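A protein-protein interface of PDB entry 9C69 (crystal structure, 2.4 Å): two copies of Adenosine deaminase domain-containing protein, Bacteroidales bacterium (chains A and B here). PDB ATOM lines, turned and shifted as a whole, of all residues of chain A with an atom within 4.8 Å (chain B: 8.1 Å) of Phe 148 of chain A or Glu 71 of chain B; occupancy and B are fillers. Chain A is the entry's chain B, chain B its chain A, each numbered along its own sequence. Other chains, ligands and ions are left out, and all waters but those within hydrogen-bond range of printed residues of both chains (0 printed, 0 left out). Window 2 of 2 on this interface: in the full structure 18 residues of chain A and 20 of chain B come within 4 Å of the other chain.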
ATOM      1  N   GLU A  18       0.655  -3.565  -9.788  1.00  0.00           N
ATOM      2  CA  GLU A  18       0.259  -2.244  -9.320  1.00  0.00           C
ATOM      3  C   GLU A  18      -1.180  -2.261  -8.809  1.00  0.00           C
ATOM      4  O   GLU A  18      -1.461  -1.820  -7.683  1.00  0.00           O
ATOM      5  CB  GLU A  18       0.442  -1.214 -10.439  1.00  0.00           C
ATOM      6  CG  GLU A  18       1.910  -0.917 -10.751  1.00  0.00           C
ATOM      7  CD  GLU A  18       2.136  -0.131 -12.045  1.00  0.00           C
ATOM      8  OE1 GLU A  18       1.166   0.424 -12.615  1.00  0.00           O
ATOM      9  OE2 GLU A  18       3.300  -0.081 -12.500  1.00  0.00           O
ATOM     10  N   ALA A  19      -2.104  -2.788  -9.620  1.00  0.00           N
ATOM     11  CA  ALA A  19      -3.509  -2.839  -9.232  1.00  0.00           C
ATOM     12  C   ALA A  19      -3.709  -3.559  -7.902  1.00  0.00           C
ATOM     13  O   ALA A  19      -4.617  -3.198  -7.142  1.00  0.00           O
ATOM     14  CB  ALA A  19      -4.328  -3.526 -10.327  1.00  0.00           C
ATOM     15  N   HIS A  21      -2.409  -3.171  -5.288  1.00  0.00           N
ATOM     16  CA  HIS A  21      -2.277  -2.233  -4.183  1.00  0.00           C
ATOM     17  C   HIS A  21      -3.365  -1.175  -4.182  1.00  0.00           C
ATOM     18  O   HIS A  21      -3.212  -0.144  -3.524  1.00  0.00           O
ATOM     19  CB  HIS A  21      -0.894  -1.569  -4.218  1.00  0.00           C
ATOM     20  CG  HIS A  21       0.237  -2.549  -4.136  1.00  0.00           C
ATOM     21  ND1 HIS A  21       0.825  -3.104  -5.257  1.00  0.00           N
ATOM     22  CD2 HIS A  21       0.866  -3.100  -3.068  1.00  0.00           C
ATOM     23  CE1 HIS A  21       1.779  -3.939  -4.884  1.00  0.00           C
ATOM     24  NE2 HIS A  21       1.822  -3.959  -3.561  1.00  0.00           N
ATOM     25  N   ALA A  22      -4.453  -1.390  -4.919  1.00  0.00           N
ATOM     26  CA  ALA A  22      -5.499  -0.374  -4.961  1.00  0.00           C
ATOM     27  C   ALA A  22      -6.182  -0.222  -3.625  1.00  0.00           C
ATOM     28  O   ALA A  22      -6.888   0.766  -3.400  1.00  0.00           O
ATOM     29  CB  ALA A  22      -6.538  -0.720  -6.018  1.00  0.00           C
ATOM     30  N   PHE A 123     -11.654   0.401 -11.492  1.00  0.00           N
ATOM     31  CA  PHE A 123     -10.635   1.429 -11.381  1.00  0.00           C
ATOM     32  C   PHE A 123      -9.570   1.233 -12.448  1.00  0.00           C
ATOM     33  O   PHE A 123      -9.393   0.137 -12.987  1.00  0.00           O
ATOM     34  CB  PHE A 123     -10.012   1.449  -9.966  1.00  0.00           C
ATOM     35  CG  PHE A 123      -9.178   0.235  -9.640  1.00  0.00           C
ATOM     36  CD1 PHE A 123      -7.823   0.214  -9.913  1.00  0.00           C
ATOM     37  CD2 PHE A 123      -9.744  -0.870  -9.008  1.00  0.00           C
ATOM     38  CE1 PHE A 123      -7.043  -0.906  -9.586  1.00  0.00           C
ATOM     39  CE2 PHE A 123      -8.975  -1.981  -8.681  1.00  0.00           C
ATOM     40  CZ  PHE A 123      -7.628  -2.004  -8.977  1.00  0.00           C
ATOM     41  N   HIS A 124      -8.897   2.333 -12.775  1.00  0.00           N
ATOM     42  CA  HIS A 124      -7.673   2.331 -13.553  1.00  0.00           C
ATOM     43  C   HIS A 124      -6.487   2.564 -12.621  1.00  0.00           C
ATOM     44  O   HIS A 124      -6.598   3.232 -11.583  1.00  0.00           O
ATOM     45  CB  HIS A 124      -7.673   3.428 -14.630  1.00  0.00           C
ATOM     46  CG  HIS A 124      -8.439   3.078 -15.865  1.00  0.00           C
ATOM     47  ND1 HIS A 124      -7.984   2.165 -16.786  1.00  0.00           N
ATOM     48  CD2 HIS A 124      -9.628   3.529 -16.334  1.00  0.00           C
ATOM     49  CE1 HIS A 124      -8.858   2.069 -17.776  1.00  0.00           C
ATOM     50  NE2 HIS A 124      -9.870   2.881 -17.521  1.00  0.00           N
ATOM     51  N   VAL A 125      -5.339   2.036 -13.025  1.00  0.00           N
ATOM     52  CA  VAL A 125      -4.090   2.286 -12.328  1.00  0.00           C
ATOM     53  C   VAL A 125      -3.172   3.026 -13.297  1.00  0.00           C
ATOM     54  O   VAL A 125      -2.980   2.590 -14.434  1.00  0.00           O
ATOM     55  CB  VAL A 125      -3.476   0.971 -11.783  1.00  0.00           C
ATOM     56  CG1 VAL A 125      -3.257  -0.084 -12.879  1.00  0.00           C
ATOM     57  CG2 VAL A 125      -2.206   1.241 -11.022  1.00  0.00           C
ATOM     58  N   ILE A 146       2.184   5.908  -8.194  1.00  0.00           N
ATOM     59  CA  ILE A 146       1.141   5.023  -8.708  1.00  0.00           C
ATOM     60  C   ILE A 146      -0.203   5.598  -8.294  1.00  0.00           C
ATOM     61  O   ILE A 146      -0.472   5.748  -7.098  1.00  0.00           O
ATOM     62  CB  ILE A 146       1.290   3.590  -8.182  1.00  0.00           C
ATOM     63  CG1 ILE A 146       2.702   3.063  -8.461  1.00  0.00           C
ATOM     64  CG2 ILE A 146       0.199   2.704  -8.760  1.00  0.00           C
ATOM     65  CD1 ILE A 146       3.006   2.864  -9.941  1.00  0.00           C
ATOM     66  N   HIS A 147      -1.048   5.899  -9.276  1.00  0.00           N
ATOM     67  CA  HIS A 147      -2.341   6.529  -9.052  1.00  0.00           C
ATOM     68  C   HIS A 147      -3.484   5.578  -9.382  1.00  0.00           C
ATOM     69  O   HIS A 147      -3.361   4.693 -10.242  1.00  0.00           O
ATOM     70  CB  HIS A 147      -2.489   7.792  -9.900  1.00  0.00           C
ATOM     71  CG  HIS A 147      -1.338   8.737  -9.776  1.00  0.00           C
ATOM     72  ND1 HIS A 147      -1.000   9.344  -8.583  1.00  0.00           N
ATOM     73  CD2 HIS A 147      -0.424   9.153 -10.686  1.00  0.00           C
ATOM     74  CE1 HIS A 147       0.060  10.110  -8.769  1.00  0.00           C
ATOM     75  NE2 HIS A 147       0.429  10.014 -10.036  1.00  0.00           N
ATOM     76  N   PHE A 148      -4.617   5.806  -8.714  1.00  0.00           N
ATOM     77  CA  PHE A 148      -5.797   4.961  -8.822  1.00  0.00           C
ATOM     78  C   PHE A 148      -6.989   5.854  -9.085  1.00  0.00           C
ATOM     79  O   PHE A 148      -7.278   6.745  -8.279  1.00  0.00           O
ATOM     80  CB  PHE A 148      -6.025   4.134  -7.545  1.00  0.00           C
ATOM     81  CG  PHE A 148      -4.888   3.228  -7.215  1.00  0.00           C
ATOM     82  CD1 PHE A 148      -4.798   1.979  -7.796  1.00  0.00           C
ATOM     83  CD2 PHE A 148      -3.860   3.657  -6.392  1.00  0.00           C
ATOM     84  CE1 PHE A 148      -3.717   1.150  -7.524  1.00  0.00           C
ATOM     85  CE2 PHE A 148      -2.782   2.837  -6.115  1.00  0.00           C
ATOM     86  CZ  PHE A 148      -2.709   1.581  -6.670  1.00  0.00           C
ATOM     87  N   ILE A 149      -7.690   5.600 -10.190  1.00  0.00           N
ATOM     88  CA  ILE A 149      -8.890   6.346 -10.557  1.00  0.00           C
ATOM     89  C   ILE A 149     -10.095   5.413 -10.462  1.00  0.00           C
ATOM     90  O   ILE A 149     -10.163   4.393 -11.160  1.00  0.00           O
ATOM     91  CB  ILE A 149      -8.775   6.950 -11.962  1.00  0.00           C
ATOM     92  CG1 ILE A 149      -7.415   7.633 -12.124  1.00  0.00           C
ATOM     93  CG2 ILE A 149      -9.902   7.948 -12.168  1.00  0.00           C
ATOM     94  CD1 ILE A 149      -7.272   8.485 -13.386  1.00  0.00           C
ATOM     95  N   GLU A 150     -11.022   5.744  -9.575  1.00  0.00           N
ATOM     96  CA  GLU A 150     -12.286   5.030  -9.466  1.00  0.00           C
ATOM     97  C   GLU A 150     -13.198   5.465 -10.612  1.00  0.00           C
ATOM     98  O   GLU A 150     -13.466   6.660 -10.765  1.00  0.00           O
ATOM     99  CB  GLU A 150     -12.929   5.331  -8.115  1.00  0.00           C
ATOM    100  CG  GLU A 150     -14.284   4.655  -7.884  1.00  0.00           C
ATOM    101  CD  GLU A 150     -14.217   3.130  -7.984  1.00  0.00           C
ATOM    102  OE1 GLU A 150     -13.421   2.509  -7.233  1.00  0.00           O
ATOM    103  OE2 GLU A 150     -14.969   2.546  -8.806  1.00  0.00           O
ATOM    104  N   ILE B  68      -5.120  12.700 -17.138  1.00  0.00           N
ATOM    105  CA  ILE B  68      -6.235  12.245 -16.325  1.00  0.00           C
ATOM    106  C   ILE B  68      -5.626  11.440 -15.183  1.00  0.00           C
ATOM    107  O   ILE B  68      -5.268  10.272 -15.349  1.00  0.00           O
ATOM    108  CB  ILE B  68      -7.249  11.441 -17.140  1.00  0.00           C
ATOM    109  CG1 ILE B  68      -8.021  12.379 -18.077  1.00  0.00           C
ATOM    110  CG2 ILE B  68      -8.224  10.755 -16.225  1.00  0.00           C
ATOM    111  CD1 ILE B  68      -8.635  11.698 -19.261  1.00  0.00           C
ATOM    112  N   LEU B  69      -5.490  12.076 -14.016  1.00  0.00           N
ATOM    113  CA  LEU B  69      -4.842  11.465 -12.861  1.00  0.00           C
ATOM    114  C   LEU B  69      -5.784  11.213 -11.697  1.00  0.00           C
ATOM    115  O   LEU B  69      -5.391  10.522 -10.753  1.00  0.00           O
ATOM    116  CB  LEU B  69      -3.679  12.346 -12.367  1.00  0.00           C
ATOM    117  CG  LEU B  69      -2.649  12.706 -13.440  1.00  0.00           C
ATOM    118  CD1 LEU B  69      -1.707  13.850 -12.999  1.00  0.00           C
ATOM    119  CD2 LEU B  69      -1.881  11.446 -13.829  1.00  0.00           C
ATOM    120  N   ASN B  70      -6.992  11.765 -11.720  1.00  0.00           N
ATOM    121  CA  ASN B  70      -7.935  11.534 -10.636  1.00  0.00           C
ATOM    122  C   ASN B  70      -9.354  11.716 -11.164  1.00  0.00           C
ATOM    123  O   ASN B  70      -9.571  12.016 -12.342  1.00  0.00           O
ATOM    124  CB  ASN B  70      -7.650  12.463  -9.455  1.00  0.00           C
ATOM    125  CG  ASN B  70      -7.638  13.918  -9.855  1.00  0.00           C
ATOM    126  OD1 ASN B  70      -8.565  14.404 -10.510  1.00  0.00           O
ATOM    127  ND2 ASN B  70      -6.592  14.631  -9.452  1.00  0.00           N
ATOM    128  N   GLU B  71     -10.323  11.557 -10.255  1.00  0.00           N
ATOM    129  CA  GLU B  71     -11.726  11.512 -10.648  1.00  0.00           C
ATOM    130  C   GLU B  71     -12.203  12.858 -11.168  1.00  0.00           C
ATOM    131  O   GLU B  71     -13.039  12.904 -12.079  1.00  0.00           O
ATOM    132  CB  GLU B  71     -12.581  11.058  -9.462  1.00  0.00           C
ATOM    133  CG  GLU B  71     -12.420   9.580  -9.074  1.00  0.00           C
ATOM    134  CD  GLU B  71     -11.109   9.275  -8.280  1.00  0.00           C
ATOM    135  OE1 GLU B  71     -10.411  10.230  -7.847  1.00  0.00           O
ATOM    136  OE2 GLU B  71     -10.783   8.078  -8.065  1.00  0.00           O
ATOM    137  N   ARG B  72     -11.690  13.958 -10.602  1.00  0.00           N
ATOM    138  CA  ARG B  72     -12.078  15.291 -11.054  1.00  0.00           C
ATOM    139  C   ARG B  72     -11.545  15.555 -12.463  1.00  0.00           C
ATOM    140  O   ARG B  72     -12.240  16.144 -13.294  1.00  0.00           O
ATOM    141  CB  ARG B  72     -11.585  16.344 -10.039  1.00  0.00           C
ATOM    142  CG  ARG B  72     -11.735  17.849 -10.429  1.00  0.00           C
ATOM    143  CD  ARG B  72     -10.491  18.428 -11.223  1.00  0.00           C
ATOM    144  NE  ARG B  72     -10.810  19.582 -12.080  1.00  0.00           N
ATOM    145  CZ  ARG B  72     -10.095  19.985 -13.132  1.00  0.00           C
ATOM    146  NH1 ARG B  72      -8.997  19.349 -13.517  1.00  0.00           N
ATOM    147  NH2 ARG B  72     -10.501  21.046 -13.827  1.00  0.00           N
ATOM    148  N   ASP B  73     -10.325  15.105 -12.755  1.00  0.00           N
ATOM    149  CA  ASP B  73      -9.793  15.235 -14.107  1.00  0.00           C
ATOM    150  C   ASP B  73     -10.665  14.495 -15.111  1.00  0.00           C
ATOM    151  O   ASP B  73     -10.987  15.024 -16.183  1.00  0.00           O
ATOM    152  CB  ASP B  73      -8.364  14.698 -14.166  1.00  0.00           C
ATOM    153  CG  ASP B  73      -7.402  15.549 -13.391  1.00  0.00           C
ATOM    154  OD1 ASP B  73      -7.744  16.720 -13.098  1.00  0.00           O
ATOM    155  OD2 ASP B  73      -6.304  15.042 -13.091  1.00  0.00           O
ATOM    156  N   PHE B  74     -11.040  13.258 -14.786  1.00  0.00           N
ATOM    157  CA  PHE B  74     -11.828  12.484 -15.724  1.00  0.00           C
ATOM    158  C   PHE B  74     -13.176  13.145 -15.954  1.00  0.00           C
ATOM    159  O   PHE B  74     -13.629  13.266 -17.105  1.00  0.00           O
ATOM    160  CB  PHE B  74     -12.011  11.046 -15.241  1.00  0.00           C
ATOM    161  CG  PHE B  74     -12.913  10.268 -16.124  1.00  0.00           C
ATOM    162  CD1 PHE B  74     -12.462   9.829 -17.365  1.00  0.00           C
ATOM    163  CD2 PHE B  74     -14.244  10.067 -15.775  1.00  0.00           C
ATOM    164  CE1 PHE B  74     -13.308   9.143 -18.224  1.00  0.00           C
ATOM    165  CE2 PHE B  74     -15.100   9.365 -16.620  1.00  0.00           C
ATOM    166  CZ  PHE B  74     -14.637   8.912 -17.852  1.00  0.00           C
ATOM    167  N   GLU B  75     -13.808  13.612 -14.874  1.00  0.00           N
ATOM    168  CA  GLU B  75     -15.103  14.274 -14.983  1.00  0.00           C
ATOM    169  C   GLU B  75     -15.006  15.535 -15.832  1.00  0.00           C
ATOM    170  O   GLU B  75     -15.871  15.798 -16.680  1.00  0.00           O
ATOM    171  CB  GLU B  75     -15.636  14.607 -13.591  1.00  0.00           C
ATOM    172  CG  GLU B  75     -17.053  15.177 -13.563  1.00  0.00           C
ATOM    173  CD  GLU B  75     -18.015  14.408 -14.461  1.00  0.00           C
ATOM    174  OE1 GLU B  75     -18.110  13.164 -14.310  1.00  0.00           O
ATOM    175  OE2 GLU B  75     -18.684  15.048 -15.303  1.00  0.00           O
ATOM    176  N   PHE B  76     -13.953  16.326 -15.629  1.00  0.00           N
ATOM    177  CA  PHE B  76     -13.798  17.520 -16.442  1.00  0.00           C
ATOM    178  C   PHE B  76     -13.565  17.149 -17.905  1.00  0.00           C
ATOM    179  O   PHE B  76     -14.145  17.761 -18.809  1.00  0.00           O
ATOM    180  CB  PHE B  76     -12.655  18.386 -15.901  1.00  0.00           C
ATOM    181  CG  PHE B  76     -12.412  19.624 -16.708  1.00  0.00           C
ATOM    182  CD1 PHE B  76     -13.399  20.600 -16.818  1.00  0.00           C
ATOM    183  CD2 PHE B  76     -11.214  19.800 -17.387  1.00  0.00           C
ATOM    184  CE1 PHE B  76     -13.188  21.743 -17.580  1.00  0.00           C
ATOM    185  CE2 PHE B  76     -10.995  20.938 -18.151  1.00  0.00           C
ATOM    186  CZ  PHE B  76     -11.982  21.908 -18.250  1.00  0.00           C
ATOM    187  N   TYR B  77     -12.742  16.125 -18.153  1.00  0.00           N
ATOM    188  CA  TYR B  77     -12.500  15.691 -19.526  1.00  0.00           C
ATOM    189  C   TYR B  77     -13.799  15.234 -20.192  1.00  0.00           C
ATOM    190  O   TYR B  77     -14.078  15.584 -21.350  1.00  0.00           O
ATOM    191  CB  TYR B  77     -11.449  14.567 -19.537  1.00  0.00           C
ATOM    192  CG  TYR B  77     -11.252  13.929 -20.894  1.00  0.00           C
ATOM    193  CD1 TYR B  77     -12.076  12.880 -21.324  1.00  0.00           C
ATOM    194  CD2 TYR B  77     -10.271  14.383 -21.762  1.00  0.00           C
ATOM    195  CE1 TYR B  77     -11.923  12.312 -22.585  1.00  0.00           C
ATOM    196  CE2 TYR B  77     -10.099  13.804 -23.013  1.00  0.00           C
ATOM    197  CZ  TYR B  77     -10.932  12.772 -23.420  1.00  0.00           C
ATOM    198  OH  TYR B  77     -10.751  12.204 -24.672  1.00  0.00           O
ATOM    199  N   GLN B  78     -14.603  14.450 -19.466  1.00  0.00           N
ATOM    200  CA  GLN B  78     -15.829  13.892 -20.025  1.00  0.00           C
ATOM    201  C   GLN B  78     -16.845  14.990 -20.334  1.00  0.00           C
ATOM    202  O   GLN B  78     -17.555  14.919 -21.351  1.00  0.00           O
ATOM    203  CB  GLN B  78     -16.411  12.853 -19.049  1.00  0.00           C
ATOM    204  CG  GLN B  78     -17.797  12.297 -19.404  1.00  0.00           C
ATOM    205  CD  GLN B  78     -17.992  10.846 -18.945  1.00  0.00           C
ATOM    206  OE1 GLN B  78     -17.466   9.911 -19.552  1.00  0.00           O
ATOM    207  NE2 GLN B  78     -18.752  10.661 -17.864  1.00  0.00           N
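The side-chain carboxylate of Glu 71 of chain B is in hydrogen-bond range of the backbone NH of Glu 150 of chain A, at 2.8 Å.
The backbone NH (N) of Leu 69 of chain B sits at hydrogen-bond distance from the side-chain carboxylate (OD2) of Asp 73 of chain B (3.2 Å). The side-chain amide oxygen (OD1) of Asn 70 of chain B lies within hydrogen-bond range of the backbone NH (N) of Arg 72 of chain B (3.2 Å). OD1 of Asn 70 of chain B sits at hydrogen-bond distance from N of Asp 73 of chain B (2.9 Å). The backbone NH of His 124 of chain A sits at hydrogen-bond distance from the backbone carbonyl oxygen of Ile 149 of chain A.
O of Phe 148 of chain A touches OE2 of Glu 71 of chain B (3.8 Å). O of Ile 68 of chain B touches CD1 of Ile 149 of chain A, 3.3 Å away. C of Leu 69 of chain B touches CD1 of Ile 149 of chain A, at 3.5 Å. CD1 of Ile 149 of chain A touches N of Asn 70 of chain B (3.7 Å). CA of Ile 149 of chain A touches OE2 of Glu 71 of chain B, 3.6 Å away.
Phe 123 of chain A touches none of the printed residues of chain B. His 147 of chain A touches none of the printed residues of chain B. Printed residues of chain B within 4 Å of Phe 148 of chain A: Glu 71. Of the printed residues of chain B, Ile 149 of chain A touches Ile 68, Leu 69, Asn 70 and Glu 71. Of the printed residues of chain B, Glu 150 of chain A touches Glu 71. Printed residues of chain A within 4 Å of Ile 68 of chain B: Ile 149 (3.3 Å). Of the printed residues of chain A, Leu 69 of chain B touches Ile 149 (3.5 Å). Of the printed residues of chain A, Asn 70 of chain B touches Ile 149. The nearest residue of chain B that does not touch Phe 148 of chain A is Leu 69 of chain B (4.9 Å). The nearest printed residue of chain A that does not touch Ile 68 of chain B is His 147 of chain A (6.6 Å).
Of the 11 printed residues of chain B, 4 touch a printed residue of chain A. Hydrophobic or aromatic side chains of chain B within 4 Å of the printed part of chain A: Ile 68. Of the 12 printed residues of chain A, 3 touch a printed residue of chain B. Along chain A the printed residues that touch a printed residue of chain B span positions 148 to 150. Among the printed residues, 6 pairs touch across the chains. Among the printed residues, no Asp or Glu carboxylate lies within 4 Å of a Lys or Arg side-chain nitrogen of the other chain.
No position is printed for both chains.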
